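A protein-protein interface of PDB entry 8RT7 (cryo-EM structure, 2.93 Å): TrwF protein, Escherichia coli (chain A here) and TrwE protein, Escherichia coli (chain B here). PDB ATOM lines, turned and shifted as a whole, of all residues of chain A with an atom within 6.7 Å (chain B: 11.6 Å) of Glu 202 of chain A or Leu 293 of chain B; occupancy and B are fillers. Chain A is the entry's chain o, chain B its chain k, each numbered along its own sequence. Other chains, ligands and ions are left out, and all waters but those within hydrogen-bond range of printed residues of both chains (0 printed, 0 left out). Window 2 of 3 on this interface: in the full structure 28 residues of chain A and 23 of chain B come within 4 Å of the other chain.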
ATOM      1  N   TYR A 194     -16.916   2.879  20.262  1.00  0.00           N
ATOM      2  CA  TYR A 194     -17.549   2.670  21.554  1.00  0.00           C
ATOM      3  C   TYR A 194     -18.136   3.965  22.086  1.00  0.00           C
ATOM      4  O   TYR A 194     -17.619   5.054  21.847  1.00  0.00           O
ATOM      5  CB  TYR A 194     -16.553   2.086  22.552  1.00  0.00           C
ATOM      6  CG  TYR A 194     -16.178   0.695  22.171  1.00  0.00           C
ATOM      7  CD1 TYR A 194     -17.066  -0.335  22.359  1.00  0.00           C
ATOM      8  CD2 TYR A 194     -14.970   0.417  21.569  1.00  0.00           C
ATOM      9  CE1 TYR A 194     -16.767  -1.596  21.989  1.00  0.00           C
ATOM     10  CE2 TYR A 194     -14.660  -0.855  21.191  1.00  0.00           C
ATOM     11  CZ  TYR A 194     -15.567  -1.856  21.409  1.00  0.00           C
ATOM     12  OH  TYR A 194     -15.281  -3.138  21.044  1.00  0.00           O
ATOM     13  N   PHE A 195     -19.228   3.813  22.822  1.00  0.00           N
ATOM     14  CA  PHE A 195     -19.974   4.913  23.415  1.00  0.00           C
ATOM     15  C   PHE A 195     -19.383   5.221  24.783  1.00  0.00           C
ATOM     16  O   PHE A 195     -19.253   4.324  25.615  1.00  0.00           O
ATOM     17  CB  PHE A 195     -21.445   4.493  23.510  1.00  0.00           C
ATOM     18  CG  PHE A 195     -22.312   5.389  24.330  1.00  0.00           C
ATOM     19  CD1 PHE A 195     -22.400   5.236  25.695  1.00  0.00           C
ATOM     20  CD2 PHE A 195     -23.114   6.326  23.725  1.00  0.00           C
ATOM     21  CE1 PHE A 195     -23.210   6.042  26.443  1.00  0.00           C
ATOM     22  CE2 PHE A 195     -23.935   7.123  24.471  1.00  0.00           C
ATOM     23  CZ  PHE A 195     -23.979   6.982  25.832  1.00  0.00           C
ATOM     24  N   VAL A 196     -19.015   6.476  25.016  1.00  0.00           N
ATOM     25  CA  VAL A 196     -18.419   6.893  26.282  1.00  0.00           C
ATOM     26  C   VAL A 196     -19.446   7.714  27.047  1.00  0.00           C
ATOM     27  O   VAL A 196     -19.974   8.700  26.525  1.00  0.00           O
ATOM     28  CB  VAL A 196     -17.128   7.693  26.071  1.00  0.00           C
ATOM     29  CG1 VAL A 196     -16.724   8.352  27.351  1.00  0.00           C
ATOM     30  CG2 VAL A 196     -16.028   6.795  25.610  1.00  0.00           C
ATOM     31  N   ASP A 197     -19.726   7.318  28.285  1.00  0.00           N
ATOM     32  CA  ASP A 197     -20.714   8.015  29.090  1.00  0.00           C
ATOM     33  C   ASP A 197     -20.042   9.090  29.943  1.00  0.00           C
ATOM     34  O   ASP A 197     -18.856   9.384  29.797  1.00  0.00           O
ATOM     35  CB  ASP A 197     -21.525   7.023  29.924  1.00  0.00           C
ATOM     36  CG  ASP A 197     -20.750   6.440  31.094  1.00  0.00           C
ATOM     37  OD1 ASP A 197     -19.541   6.691  31.229  1.00  0.00           O
ATOM     38  OD2 ASP A 197     -21.370   5.726  31.903  1.00  0.00           O
ATOM     39  N   GLY A 200     -16.902   8.254  31.945  1.00  0.00           N
ATOM     40  CA  GLY A 200     -15.812   7.665  31.206  1.00  0.00           C
ATOM     41  C   GLY A 200     -15.949   6.194  30.903  1.00  0.00           C
ATOM     42  O   GLY A 200     -14.987   5.591  30.425  1.00  0.00           O
ATOM     43  N   ASN A 201     -17.103   5.597  31.167  1.00  0.00           N
ATOM     44  CA  ASN A 201     -17.302   4.187  30.880  1.00  0.00           C
ATOM     45  C   ASN A 201     -17.692   3.988  29.426  1.00  0.00           C
ATOM     46  O   ASN A 201     -18.487   4.746  28.869  1.00  0.00           O
ATOM     47  CB  ASN A 201     -18.377   3.594  31.786  1.00  0.00           C
ATOM     48  CG  ASN A 201     -18.057   3.754  33.245  1.00  0.00           C
ATOM     49  OD1 ASN A 201     -17.044   3.256  33.726  1.00  0.00           O
ATOM     50  ND2 ASN A 201     -18.929   4.434  33.967  1.00  0.00           N
ATOM     51  N   GLU A 202     -17.146   2.943  28.824  1.00  0.00           N
ATOM     52  CA  GLU A 202     -17.372   2.634  27.426  1.00  0.00           C
ATOM     53  C   GLU A 202     -18.406   1.526  27.322  1.00  0.00           C
ATOM     54  O   GLU A 202     -18.407   0.596  28.130  1.00  0.00           O
ATOM     55  CB  GLU A 202     -16.079   2.178  26.769  1.00  0.00           C
ATOM     56  CG  GLU A 202     -15.021   3.221  26.715  1.00  0.00           C
ATOM     57  CD  GLU A 202     -13.760   2.688  26.116  1.00  0.00           C
ATOM     58  OE1 GLU A 202     -13.709   1.479  25.825  1.00  0.00           O
ATOM     59  OE2 GLU A 202     -12.796   3.457  25.995  1.00  0.00           O
ATOM     60  N   SER A 203     -19.277   1.619  26.324  1.00  0.00           N
ATOM     61  CA  SER A 203     -20.284   0.594  26.130  1.00  0.00           C
ATOM     62  C   SER A 203     -20.580   0.451  24.649  1.00  0.00           C
ATOM     63  O   SER A 203     -20.267   1.326  23.844  1.00  0.00           O
ATOM     64  CB  SER A 203     -21.562   0.906  26.910  1.00  0.00           C
ATOM     65  OG  SER A 203     -22.166   2.110  26.480  1.00  0.00           O
ATOM     66  N   LEU A 204     -21.195  -0.673  24.303  1.00  0.00           N
ATOM     67  CA  LEU A 204     -21.490  -0.969  22.915  1.00  0.00           C
ATOM     68  C   LEU A 204     -22.582  -0.056  22.386  1.00  0.00           C
ATOM     69  O   LEU A 204     -23.445   0.415  23.124  1.00  0.00           O
ATOM     70  CB  LEU A 204     -21.910  -2.426  22.756  1.00  0.00           C
ATOM     71  CG  LEU A 204     -21.027  -3.464  23.430  1.00  0.00           C
ATOM     72  CD1 LEU A 204     -21.681  -4.806  23.376  1.00  0.00           C
ATOM     73  CD2 LEU A 204     -19.695  -3.524  22.754  1.00  0.00           C
ATOM     74  N   MET A 227     -15.210   6.638  21.597  1.00  0.00           N
ATOM     75  CA  MET A 227     -13.915   5.988  21.709  1.00  0.00           C
ATOM     76  C   MET A 227     -13.744   5.020  20.556  1.00  0.00           C
ATOM     77  O   MET A 227     -14.627   4.203  20.296  1.00  0.00           O
ATOM     78  CB  MET A 227     -13.771   5.246  23.033  1.00  0.00           C
ATOM     79  CG  MET A 227     -12.489   4.474  23.158  1.00  0.00           C
ATOM     80  SD  MET A 227     -11.020   5.499  23.223  1.00  0.00           S
ATOM     81  CE  MET A 227     -11.357   6.454  24.679  1.00  0.00           C
ATOM     82  N   ILE A 228     -12.603   5.103  19.884  1.00  0.00           N
ATOM     83  CA  ILE A 228     -12.279   4.277  18.729  1.00  0.00           C
ATOM     84  C   ILE A 228     -11.099   3.395  19.101  1.00  0.00           C
ATOM     85  O   ILE A 228     -10.075   3.895  19.571  1.00  0.00           O
ATOM     86  CB  ILE A 228     -11.948   5.145  17.506  1.00  0.00           C
ATOM     87  CG1 ILE A 228     -13.174   5.932  17.063  1.00  0.00           C
ATOM     88  CG2 ILE A 228     -11.454   4.296  16.392  1.00  0.00           C
ATOM     89  CD1 ILE A 228     -12.992   6.640  15.768  1.00  0.00           C
ATOM     90  N   ARG A 229     -11.238   2.090  18.898  1.00  0.00           N
ATOM     91  CA  ARG A 229     -10.202   1.137  19.268  1.00  0.00           C
ATOM     92  C   ARG A 229      -9.953   0.153  18.137  1.00  0.00           C
ATOM     93  O   ARG A 229     -10.894  -0.339  17.518  1.00  0.00           O
ATOM     94  CB  ARG A 229     -10.588   0.371  20.526  1.00  0.00           C
ATOM     95  CG  ARG A 229     -10.827   1.239  21.728  1.00  0.00           C
ATOM     96  CD  ARG A 229     -11.031   0.406  22.958  1.00  0.00           C
ATOM     97  NE  ARG A 229     -11.086   1.217  24.162  1.00  0.00           N
ATOM     98  CZ  ARG A 229     -10.019   1.682  24.793  1.00  0.00           C
ATOM     99  NH1 ARG A 229      -8.812   1.426  24.332  1.00  0.00           N
ATOM    100  NH2 ARG A 229     -10.162   2.407  25.885  1.00  0.00           N
ATOM    101  N   ALA A 234      -5.911   3.346  20.618  1.00  0.00           N
ATOM    102  CA  ALA A 234      -7.149   3.982  21.030  1.00  0.00           C
ATOM    103  C   ALA A 234      -7.145   5.441  20.605  1.00  0.00           C
ATOM    104  O   ALA A 234      -6.108   6.104  20.635  1.00  0.00           O
ATOM    105  CB  ALA A 234      -7.342   3.873  22.533  1.00  0.00           C
ATOM    106  N   GLY B 210     -26.353 -10.805  16.922  1.00  0.00           N
ATOM    107  CA  GLY B 210     -25.241  -9.967  17.275  1.00  0.00           C
ATOM    108  C   GLY B 210     -25.566  -8.504  17.360  1.00  0.00           C
ATOM    109  O   GLY B 210     -24.648  -7.687  17.457  1.00  0.00           O
ATOM    110  N   THR B 211     -26.839  -8.143  17.300  1.00  0.00           N
ATOM    111  CA  THR B 211     -27.240  -6.765  17.514  1.00  0.00           C
ATOM    112  C   THR B 211     -27.317  -6.505  19.006  1.00  0.00           C
ATOM    113  O   THR B 211     -27.874  -7.307  19.756  1.00  0.00           O
ATOM    114  CB  THR B 211     -28.579  -6.481  16.845  1.00  0.00           C
ATOM    115  OG1 THR B 211     -28.476  -6.760  15.449  1.00  0.00           O
ATOM    116  CG2 THR B 211     -28.959  -5.038  17.024  1.00  0.00           C
ATOM    117  N   GLN B 212     -26.737  -5.395  19.437  1.00  0.00           N
ATOM    118  CA  GLN B 212     -26.657  -5.064  20.848  1.00  0.00           C
ATOM    119  C   GLN B 212     -27.811  -4.148  21.217  1.00  0.00           C
ATOM    120  O   GLN B 212     -27.939  -3.049  20.672  1.00  0.00           O
ATOM    121  CB  GLN B 212     -25.324  -4.397  21.168  1.00  0.00           C
ATOM    122  CG  GLN B 212     -24.126  -5.083  20.558  1.00  0.00           C
ATOM    123  CD  GLN B 212     -23.859  -6.446  21.161  1.00  0.00           C
ATOM    124  OE1 GLN B 212     -24.267  -6.731  22.278  1.00  0.00           O
ATOM    125  NE2 GLN B 212     -23.168  -7.292  20.421  1.00  0.00           N
ATOM    126  N   LEU B 213     -28.636  -4.598  22.149  1.00  0.00           N
ATOM    127  CA  LEU B 213     -29.738  -3.817  22.679  1.00  0.00           C
ATOM    128  C   LEU B 213     -29.291  -3.262  24.018  1.00  0.00           C
ATOM    129  O   LEU B 213     -28.936  -4.023  24.916  1.00  0.00           O
ATOM    130  CB  LEU B 213     -30.980  -4.683  22.858  1.00  0.00           C
ATOM    131  CG  LEU B 213     -31.989  -4.933  21.747  1.00  0.00           C
ATOM    132  CD1 LEU B 213     -31.318  -5.368  20.488  1.00  0.00           C
ATOM    133  CD2 LEU B 213     -32.938  -6.000  22.211  1.00  0.00           C
ATOM    134  N   ASP B 214     -29.303  -1.946  24.153  1.00  0.00           N
ATOM    135  CA  ASP B 214     -28.882  -1.304  25.388  1.00  0.00           C
ATOM    136  C   ASP B 214     -30.107  -1.028  26.239  1.00  0.00           C
ATOM    137  O   ASP B 214     -31.005  -0.297  25.816  1.00  0.00           O
ATOM    138  CB  ASP B 214     -28.139  -0.006  25.099  1.00  0.00           C
ATOM    139  CG  ASP B 214     -27.507   0.581  26.329  1.00  0.00           C
ATOM    140  OD1 ASP B 214     -28.051   1.563  26.866  1.00  0.00           O
ATOM    141  OD2 ASP B 214     -26.462   0.059  26.762  1.00  0.00           O
ATOM    142  N   CYS B 215     -30.145  -1.609  27.428  1.00  0.00           N
ATOM    143  CA  CYS B 215     -31.249  -1.408  28.343  1.00  0.00           C
ATOM    144  C   CYS B 215     -30.706  -1.168  29.741  1.00  0.00           C
ATOM    145  O   CYS B 215     -29.593  -1.562  30.069  1.00  0.00           O
ATOM    146  CB  CYS B 215     -32.226  -2.591  28.301  1.00  0.00           C
ATOM    147  SG  CYS B 215     -31.740  -4.098  29.118  1.00  0.00           S
ATOM    148  N   ARG B 235     -32.603   3.196  24.321  1.00  0.00           N
ATOM    149  CA  ARG B 235     -32.447   3.781  23.003  1.00  0.00           C
ATOM    150  C   ARG B 235     -33.326   3.055  22.002  1.00  0.00           C
ATOM    151  O   ARG B 235     -33.678   1.892  22.183  1.00  0.00           O
ATOM    152  CB  ARG B 235     -30.999   3.703  22.521  1.00  0.00           C
ATOM    153  CG  ARG B 235     -30.009   4.442  23.363  1.00  0.00           C
ATOM    154  CD  ARG B 235     -28.717   4.600  22.629  1.00  0.00           C
ATOM    155  NE  ARG B 235     -27.771   3.522  22.877  1.00  0.00           N
ATOM    156  CZ  ARG B 235     -26.797   3.580  23.774  1.00  0.00           C
ATOM    157  NH1 ARG B 235     -25.971   2.564  23.919  1.00  0.00           N
ATOM    158  NH2 ARG B 235     -26.658   4.648  24.535  1.00  0.00           N
ATOM    159  N   ARG B 267     -20.087 -13.937  37.754  1.00  0.00           N
ATOM    160  CA  ARG B 267     -21.074 -13.501  36.782  1.00  0.00           C
ATOM    161  C   ARG B 267     -22.137 -14.572  36.647  1.00  0.00           C
ATOM    162  O   ARG B 267     -21.820 -15.757  36.570  1.00  0.00           O
ATOM    163  CB  ARG B 267     -20.446 -13.232  35.420  1.00  0.00           C
ATOM    164  CG  ARG B 267     -19.435 -12.140  35.430  1.00  0.00           C
ATOM    165  CD  ARG B 267     -19.036 -11.758  34.049  1.00  0.00           C
ATOM    166  NE  ARG B 267     -19.952 -10.803  33.458  1.00  0.00           N
ATOM    167  CZ  ARG B 267     -19.824  -9.492  33.568  1.00  0.00           C
ATOM    168  NH1 ARG B 267     -18.827  -8.986  34.264  1.00  0.00           N
ATOM    169  NH2 ARG B 267     -20.700  -8.691  32.995  1.00  0.00           N
ATOM    170  N   PRO B 288     -28.942 -14.057  25.315  1.00  0.00           N
ATOM    171  CA  PRO B 288     -28.113 -13.898  26.506  1.00  0.00           C
ATOM    172  C   PRO B 288     -28.012 -12.448  26.942  1.00  0.00           C
ATOM    173  O   PRO B 288     -27.852 -11.538  26.130  1.00  0.00           O
ATOM    174  CB  PRO B 288     -26.756 -14.436  26.048  1.00  0.00           C
ATOM    175  CG  PRO B 288     -26.762 -14.249  24.612  1.00  0.00           C
ATOM    176  CD  PRO B 288     -28.143 -14.490  24.161  1.00  0.00           C
ATOM    177  N   GLY B 289     -28.102 -12.239  28.248  1.00  0.00           N
ATOM    178  CA  GLY B 289     -27.867 -10.933  28.818  1.00  0.00           C
ATOM    179  C   GLY B 289     -26.406 -10.783  29.195  1.00  0.00           C
ATOM    180  O   GLY B 289     -25.795 -11.696  29.736  1.00  0.00           O
ATOM    181  N   THR B 290     -25.853  -9.621  28.881  1.00  0.00           N
ATOM    182  CA  THR B 290     -24.435  -9.362  29.029  1.00  0.00           C
ATOM    183  C   THR B 290     -24.241  -8.072  29.814  1.00  0.00           C
ATOM    184  O   THR B 290     -25.197  -7.454  30.278  1.00  0.00           O
ATOM    185  CB  THR B 290     -23.752  -9.292  27.657  1.00  0.00           C
ATOM    186  OG1 THR B 290     -24.142  -8.096  26.985  1.00  0.00           O
ATOM    187  CG2 THR B 290     -24.143 -10.471  26.804  1.00  0.00           C
ATOM    188  N   GLY B 291     -22.990  -7.677  29.984  1.00  0.00           N
ATOM    189  CA  GLY B 291     -22.666  -6.430  30.626  1.00  0.00           C
ATOM    190  C   GLY B 291     -22.625  -5.304  29.623  1.00  0.00           C
ATOM    191  O   GLY B 291     -22.927  -5.493  28.447  1.00  0.00           O
ATOM    192  N   PRO B 292     -22.246  -4.107  30.067  1.00  0.00           N
ATOM    193  CA  PRO B 292     -22.263  -2.950  29.162  1.00  0.00           C
ATOM    194  C   PRO B 292     -21.346  -3.089  27.965  1.00  0.00           C
ATOM    195  O   PRO B 292     -21.588  -2.443  26.943  1.00  0.00           O
ATOM    196  CB  PRO B 292     -21.821  -1.795  30.064  1.00  0.00           C
ATOM    197  CG  PRO B 292     -22.057  -2.267  31.425  1.00  0.00           C
ATOM    198  CD  PRO B 292     -21.828  -3.726  31.419  1.00  0.00           C
ATOM    199  N   LEU B 293     -20.300  -3.905  28.055  1.00  0.00           N
ATOM    200  CA  LEU B 293     -19.375  -4.115  26.954  1.00  0.00           C
ATOM    201  C   LEU B 293     -19.474  -5.519  26.381  1.00  0.00           C
ATOM    202  O   LEU B 293     -18.550  -5.975  25.713  1.00  0.00           O
ATOM    203  CB  LEU B 293     -17.944  -3.828  27.392  1.00  0.00           C
ATOM    204  CG  LEU B 293     -17.500  -2.385  27.231  1.00  0.00           C
ATOM    205  CD1 LEU B 293     -16.193  -2.183  27.919  1.00  0.00           C
ATOM    206  CD2 LEU B 293     -17.393  -2.042  25.773  1.00  0.00           C
ATOM    207  N   GLY B 294     -20.567  -6.217  26.640  1.00  0.00           N
ATOM    208  CA  GLY B 294     -20.822  -7.469  25.977  1.00  0.00           C
ATOM    209  C   GLY B 294     -20.199  -8.687  26.603  1.00  0.00           C
ATOM    210  O   GLY B 294     -20.107  -9.717  25.934  1.00  0.00           O
ATOM    211  N   GLU B 295     -19.767  -8.619  27.853  1.00  0.00           N
ATOM    212  CA  GLU B 295     -19.185  -9.776  28.505  1.00  0.00           C
ATOM    213  C   GLU B 295     -20.292 -10.620  29.115  1.00  0.00           C
ATOM    214  O   GLU B 295     -21.232 -10.095  29.706  1.00  0.00           O
ATOM    215  CB  GLU B 295     -18.163  -9.355  29.557  1.00  0.00           C
ATOM    216  CG  GLU B 295     -18.643  -8.344  30.543  1.00  0.00           C
ATOM    217  CD  GLU B 295     -18.348  -6.928  30.138  1.00  0.00           C
ATOM    218  OE1 GLU B 295     -18.841  -6.513  29.086  1.00  0.00           O
ATOM    219  OE2 GLU B 295     -17.642  -6.219  30.871  1.00  0.00           O
ATOM    220  N   ALA B 296     -20.175 -11.931  28.950  1.00  0.00           N
ATOM    221  CA  ALA B 296     -21.300 -12.826  29.165  1.00  0.00           C
ATOM    222  C   ALA B 296     -21.765 -12.809  30.608  1.00  0.00           C
ATOM    223  O   ALA B 296     -20.967 -12.924  31.538  1.00  0.00           O
ATOM    224  CB  ALA B 296     -20.913 -14.243  28.772  1.00  0.00           C
ATOM    225  N   GLY B 297     -23.069 -12.701  30.786  1.00  0.00           N
ATOM    226  CA  GLY B 297     -23.661 -12.712  32.099  1.00  0.00           C
ATOM    227  C   GLY B 297     -23.618 -11.352  32.762  1.00  0.00           C
ATOM    228  O   GLY B 297     -22.879 -10.454  32.376  1.00  0.00           O
ATOM    229  N   LEU B 298     -24.431 -11.212  33.795  1.00  0.00           N
ATOM    230  CA  LEU B 298     -24.468 -10.004  34.597  1.00  0.00           C
ATOM    231  C   LEU B 298     -23.585 -10.197  35.817  1.00  0.00           C
ATOM    232  O   LEU B 298     -23.537 -11.285  36.387  1.00  0.00           O
ATOM    233  CB  LEU B 298     -25.895  -9.684  35.035  1.00  0.00           C
ATOM    234  CG  LEU B 298     -26.770  -8.806  34.153  1.00  0.00           C
ATOM    235  CD1 LEU B 298     -27.030  -9.485  32.858  1.00  0.00           C
ATOM    236  CD2 LEU B 298     -28.072  -8.555  34.849  1.00  0.00           C
ATOM    237  N   GLY B 299     -22.885  -9.150  36.215  1.00  0.00           N
ATOM    238  CA  GLY B 299     -22.032  -9.268  37.371  1.00  0.00           C
ATOM    239  C   GLY B 299     -21.978  -8.021  38.217  1.00  0.00           C
ATOM    240  O   GLY B 299     -21.933  -6.911  37.691  1.00  0.00           O
ATOM    241  N   LYS B 367     -26.306  -7.151  42.376  1.00  0.00           N
ATOM    242  CA  LYS B 367     -26.230  -6.133  41.344  1.00  0.00           C
ATOM    243  C   LYS B 367     -27.264  -5.070  41.655  1.00  0.00           C
ATOM    244  O   LYS B 367     -28.414  -5.393  41.946  1.00  0.00           O
ATOM    245  CB  LYS B 367     -26.473  -6.732  39.966  1.00  0.00           C
ATOM    246  CG  LYS B 367     -26.103  -5.818  38.842  1.00  0.00           C
ATOM    247  CD  LYS B 367     -26.047  -6.556  37.547  1.00  0.00           C
ATOM    248  CE  LYS B 367     -25.861  -5.588  36.417  1.00  0.00           C
ATOM    249  NZ  LYS B 367     -24.754  -4.662  36.717  1.00  0.00           N
ATOM    250  N   GLU B 371     -28.437  -0.231  36.731  1.00  0.00           N
ATOM    251  CA  GLU B 371     -27.196  -0.590  36.070  1.00  0.00           C
ATOM    252  C   GLU B 371     -27.433  -0.830  34.591  1.00  0.00           C
ATOM    253  O   GLU B 371     -28.466  -1.365  34.193  1.00  0.00           O
ATOM    254  CB  GLU B 371     -26.608  -1.838  36.710  1.00  0.00           C
ATOM    255  CG  GLU B 371     -26.166  -1.645  38.131  1.00  0.00           C
ATOM    256  CD  GLU B 371     -24.999  -0.700  38.243  1.00  0.00           C
ATOM    257  OE1 GLU B 371     -24.174  -0.661  37.307  1.00  0.00           O
ATOM    258  OE2 GLU B 371     -24.905   0.016  39.262  1.00  0.00           O
ATOM    259  N   ARG B 372     -26.468  -0.439  33.775  1.00  0.00           N
ATOM    260  CA  ARG B 372     -26.587  -0.584  32.336  1.00  0.00           C
ATOM    261  C   ARG B 372     -26.215  -1.998  31.919  1.00  0.00           C
ATOM    262  O   ARG B 372     -25.213  -2.544  32.382  1.00  0.00           O
ATOM    263  CB  ARG B 372     -25.689   0.422  31.634  1.00  0.00           C
ATOM    264  CG  ARG B 372     -26.273   0.999  30.385  1.00  0.00           C
ATOM    265  CD  ARG B 372     -25.226   1.771  29.625  1.00  0.00           C
ATOM    266  NE  ARG B 372     -25.108   3.148  30.078  1.00  0.00           N
ATOM    267  CZ  ARG B 372     -25.686   4.180  29.480  1.00  0.00           C
ATOM    268  NH1 ARG B 372     -25.515   5.401  29.959  1.00  0.00           N
ATOM    269  NH2 ARG B 372     -26.436   3.994  28.409  1.00  0.00           N
ATOM    270  N   VAL B 373     -27.025  -2.594  31.051  1.00  0.00           N
ATOM    271  CA  VAL B 373     -26.808  -3.951  30.575  1.00  0.00           C
ATOM    272  C   VAL B 373     -27.039  -3.974  29.069  1.00  0.00           C
ATOM    273  O   VAL B 373     -27.512  -3.008  28.480  1.00  0.00           O
ATOM    274  CB  VAL B 373     -27.715  -4.970  31.297  1.00  0.00           C
ATOM    275  CG1 VAL B 373     -27.352  -5.051  32.747  1.00  0.00           C
ATOM    276  CG2 VAL B 373     -29.137  -4.569  31.198  1.00  0.00           C
ATOM    277  N   ASN B 374     -26.675  -5.087  28.443  1.00  0.00           N
ATOM    278  CA  ASN B 374     -26.955  -5.325  27.036  1.00  0.00           C
ATOM    279  C   ASN B 374     -27.694  -6.638  26.872  1.00  0.00           C
ATOM    280  O   ASN B 374     -27.598  -7.540  27.700  1.00  0.00           O
ATOM    281  CB  ASN B 374     -25.700  -5.389  26.149  1.00  0.00           C
ATOM    282  CG  ASN B 374     -25.025  -4.059  25.976  1.00  0.00           C
ATOM    283  OD1 ASN B 374     -25.670  -3.035  25.793  1.00  0.00           O
ATOM    284  ND2 ASN B 374     -23.710  -4.073  25.986  1.00  0.00           N
ATOM    285  N   ILE B 375     -28.432  -6.727  25.776  1.00  0.00           N
ATOM    286  CA  ILE B 375     -28.956  -7.982  25.265  1.00  0.00           C
ATOM    287  C   ILE B 375     -28.302  -8.204  23.915  1.00  0.00           C
ATOM    288  O   ILE B 375     -28.426  -7.366  23.019  1.00  0.00           O
ATOM    289  CB  ILE B 375     -30.485  -7.954  25.148  1.00  0.00           C
ATOM    290  CG1 ILE B 375     -31.093  -7.361  26.411  1.00  0.00           C
ATOM    291  CG2 ILE B 375     -31.032  -9.337  24.914  1.00  0.00           C
ATOM    292  CD1 ILE B 375     -32.495  -6.942  26.243  1.00  0.00           C
ATOM    293  N   LEU B 376     -27.575  -9.305  23.781  1.00  0.00           N
ATOM    294  CA  LEU B 376     -26.967  -9.678  22.513  1.00  0.00           C
ATOM    295  C   LEU B 376     -27.944 -10.602  21.813  1.00  0.00           C
ATOM    296  O   LEU B 376     -28.134 -11.741  22.236  1.00  0.00           O
ATOM    297  CB  LEU B 376     -25.619 -10.358  22.727  1.00  0.00           C
ATOM    298  CG  LEU B 376     -24.657 -10.484  21.544  1.00  0.00           C
ATOM    299  CD1 LEU B 376     -23.233 -10.419  22.033  1.00  0.00           C
ATOM    300  CD2 LEU B 376     -24.872 -11.763  20.778  1.00  0.00           C
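NH1 of Arg 235 of chain B is in hydrogen-bond range of O of Leu 204 of chain A, 3.4 Å away. The backbone carbonyl oxygen (O) of Pro 292 of chain B is in hydrogen-bond range of the backbone NH (N) of Leu 204 of chain A, 3.2 Å away.
The side-chain carboxylate (OD1) of Asp 214 of chain B is in salt-bridge range of the guanidinium group (NH1) of Arg 235 of chain B (3.7 Å). O of Asn 374 of chain B sits at hydrogen-bond distance from N of Thr 290 of chain B. The backbone carbonyl oxygen (O) of Gly 291 of chain B sits at hydrogen-bond distance from the side-chain amide nitrogen (ND2) of Asn 374 of chain B, 2.9 Å away. The backbone NH of Leu 293 of chain B lies close to the side-chain carboxylate of Glu 295 of chain B. The backbone carbonyl oxygen (O) of Phe 195 of chain A lies within hydrogen-bond range of the backbone NH (N) of Ser 203 of chain A (2.8 Å). The guanidinium group (NH2) of Arg 229 of chain A is in salt-bridge range of the side-chain carboxylate (OE2) of Glu 202 of chain A (2.8 Å).
Leu 293 of chain B touches Tyr 194 of chain A. CE2 of Phe 195 of chain A touches NH2 of Arg 235 of chain B (3.7 Å). Leu 293 of chain B touches Glu 202 of chain A (CG to O, 3.2 Å). CB of Ser 203 of chain A touches O of Pro 292 of chain B, at 3.3 Å. Leu 293 of chain B touches Ser 203 of chain A (CD2 to CA, 3.9 Å). Gln 212 of chain B touches Leu 204 of chain A. CD1 of Leu 204 of chain A touches C of Leu 293 of chain B, at 3.8 Å. Gly 294 of chain B touches Leu 204 of chain A (N to CD1, 3.7 Å). CD1 of Leu 204 of chain A touches ND2 of Asn 374 of chain B, at 3.4 Å.
Tyr 194 of chain A touches one residue of chain B. Of the printed residues of chain B, Phe 195 of chain A touches Arg 235. No residue of chain B comes within 4 Å of Val 196 of chain A. No residue of chain B comes within 4 Å of Asp 197 of chain A. No residue of chain B comes within 4 Å of Gly 200 of chain A. No residue of chain B comes within 4 Å of Asn 201 of chain A. Glu 202 of chain A touches one residue of chain B. Of the printed residues of chain B, Ser 203 of chain A touches Pro 292 and Leu 293. Of chain B, only Gln 212, Arg 235, Pro 292, Leu 293, Gly 294 and Asn 374 come within 4 Å of Leu 204 of chain A. No residue of chain B comes within 4 Å of Met 227 of chain A. Printed residues of chain A within 4 Å of Pro 292 of chain B: Ser 203 and Leu 204. Of chain A, only Tyr 194, Glu 202, Ser 203 and Leu 204 come within 4 Å of Leu 293 of chain B. Of the printed residues of chain A, Gly 294 of chain B touches Leu 204 (3.7 Å). Arg 372 of chain B touches none of the printed residues of chain A. The nearest residue of chain B that does not touch Glu 202 of chain A is Pro 292 of chain B (4.6 Å). The nearest residue of chain A that does not touch Leu 293 of chain B is Asn 201 of chain A (6.5 Å).
Of the 27 printed residues of chain B, 6 touch a printed residue of chain A. Hydrophobic or aromatic side chains of chain B within 4 Å of the printed part of chain A: Leu 293. Of the 13 printed residues of chain A, 5 touch a printed residue of chain B. Among the printed residues, no Asp or Glu carboxylate lies within 4 Å of a Lys or Arg side-chain nitrogen of the other chain.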
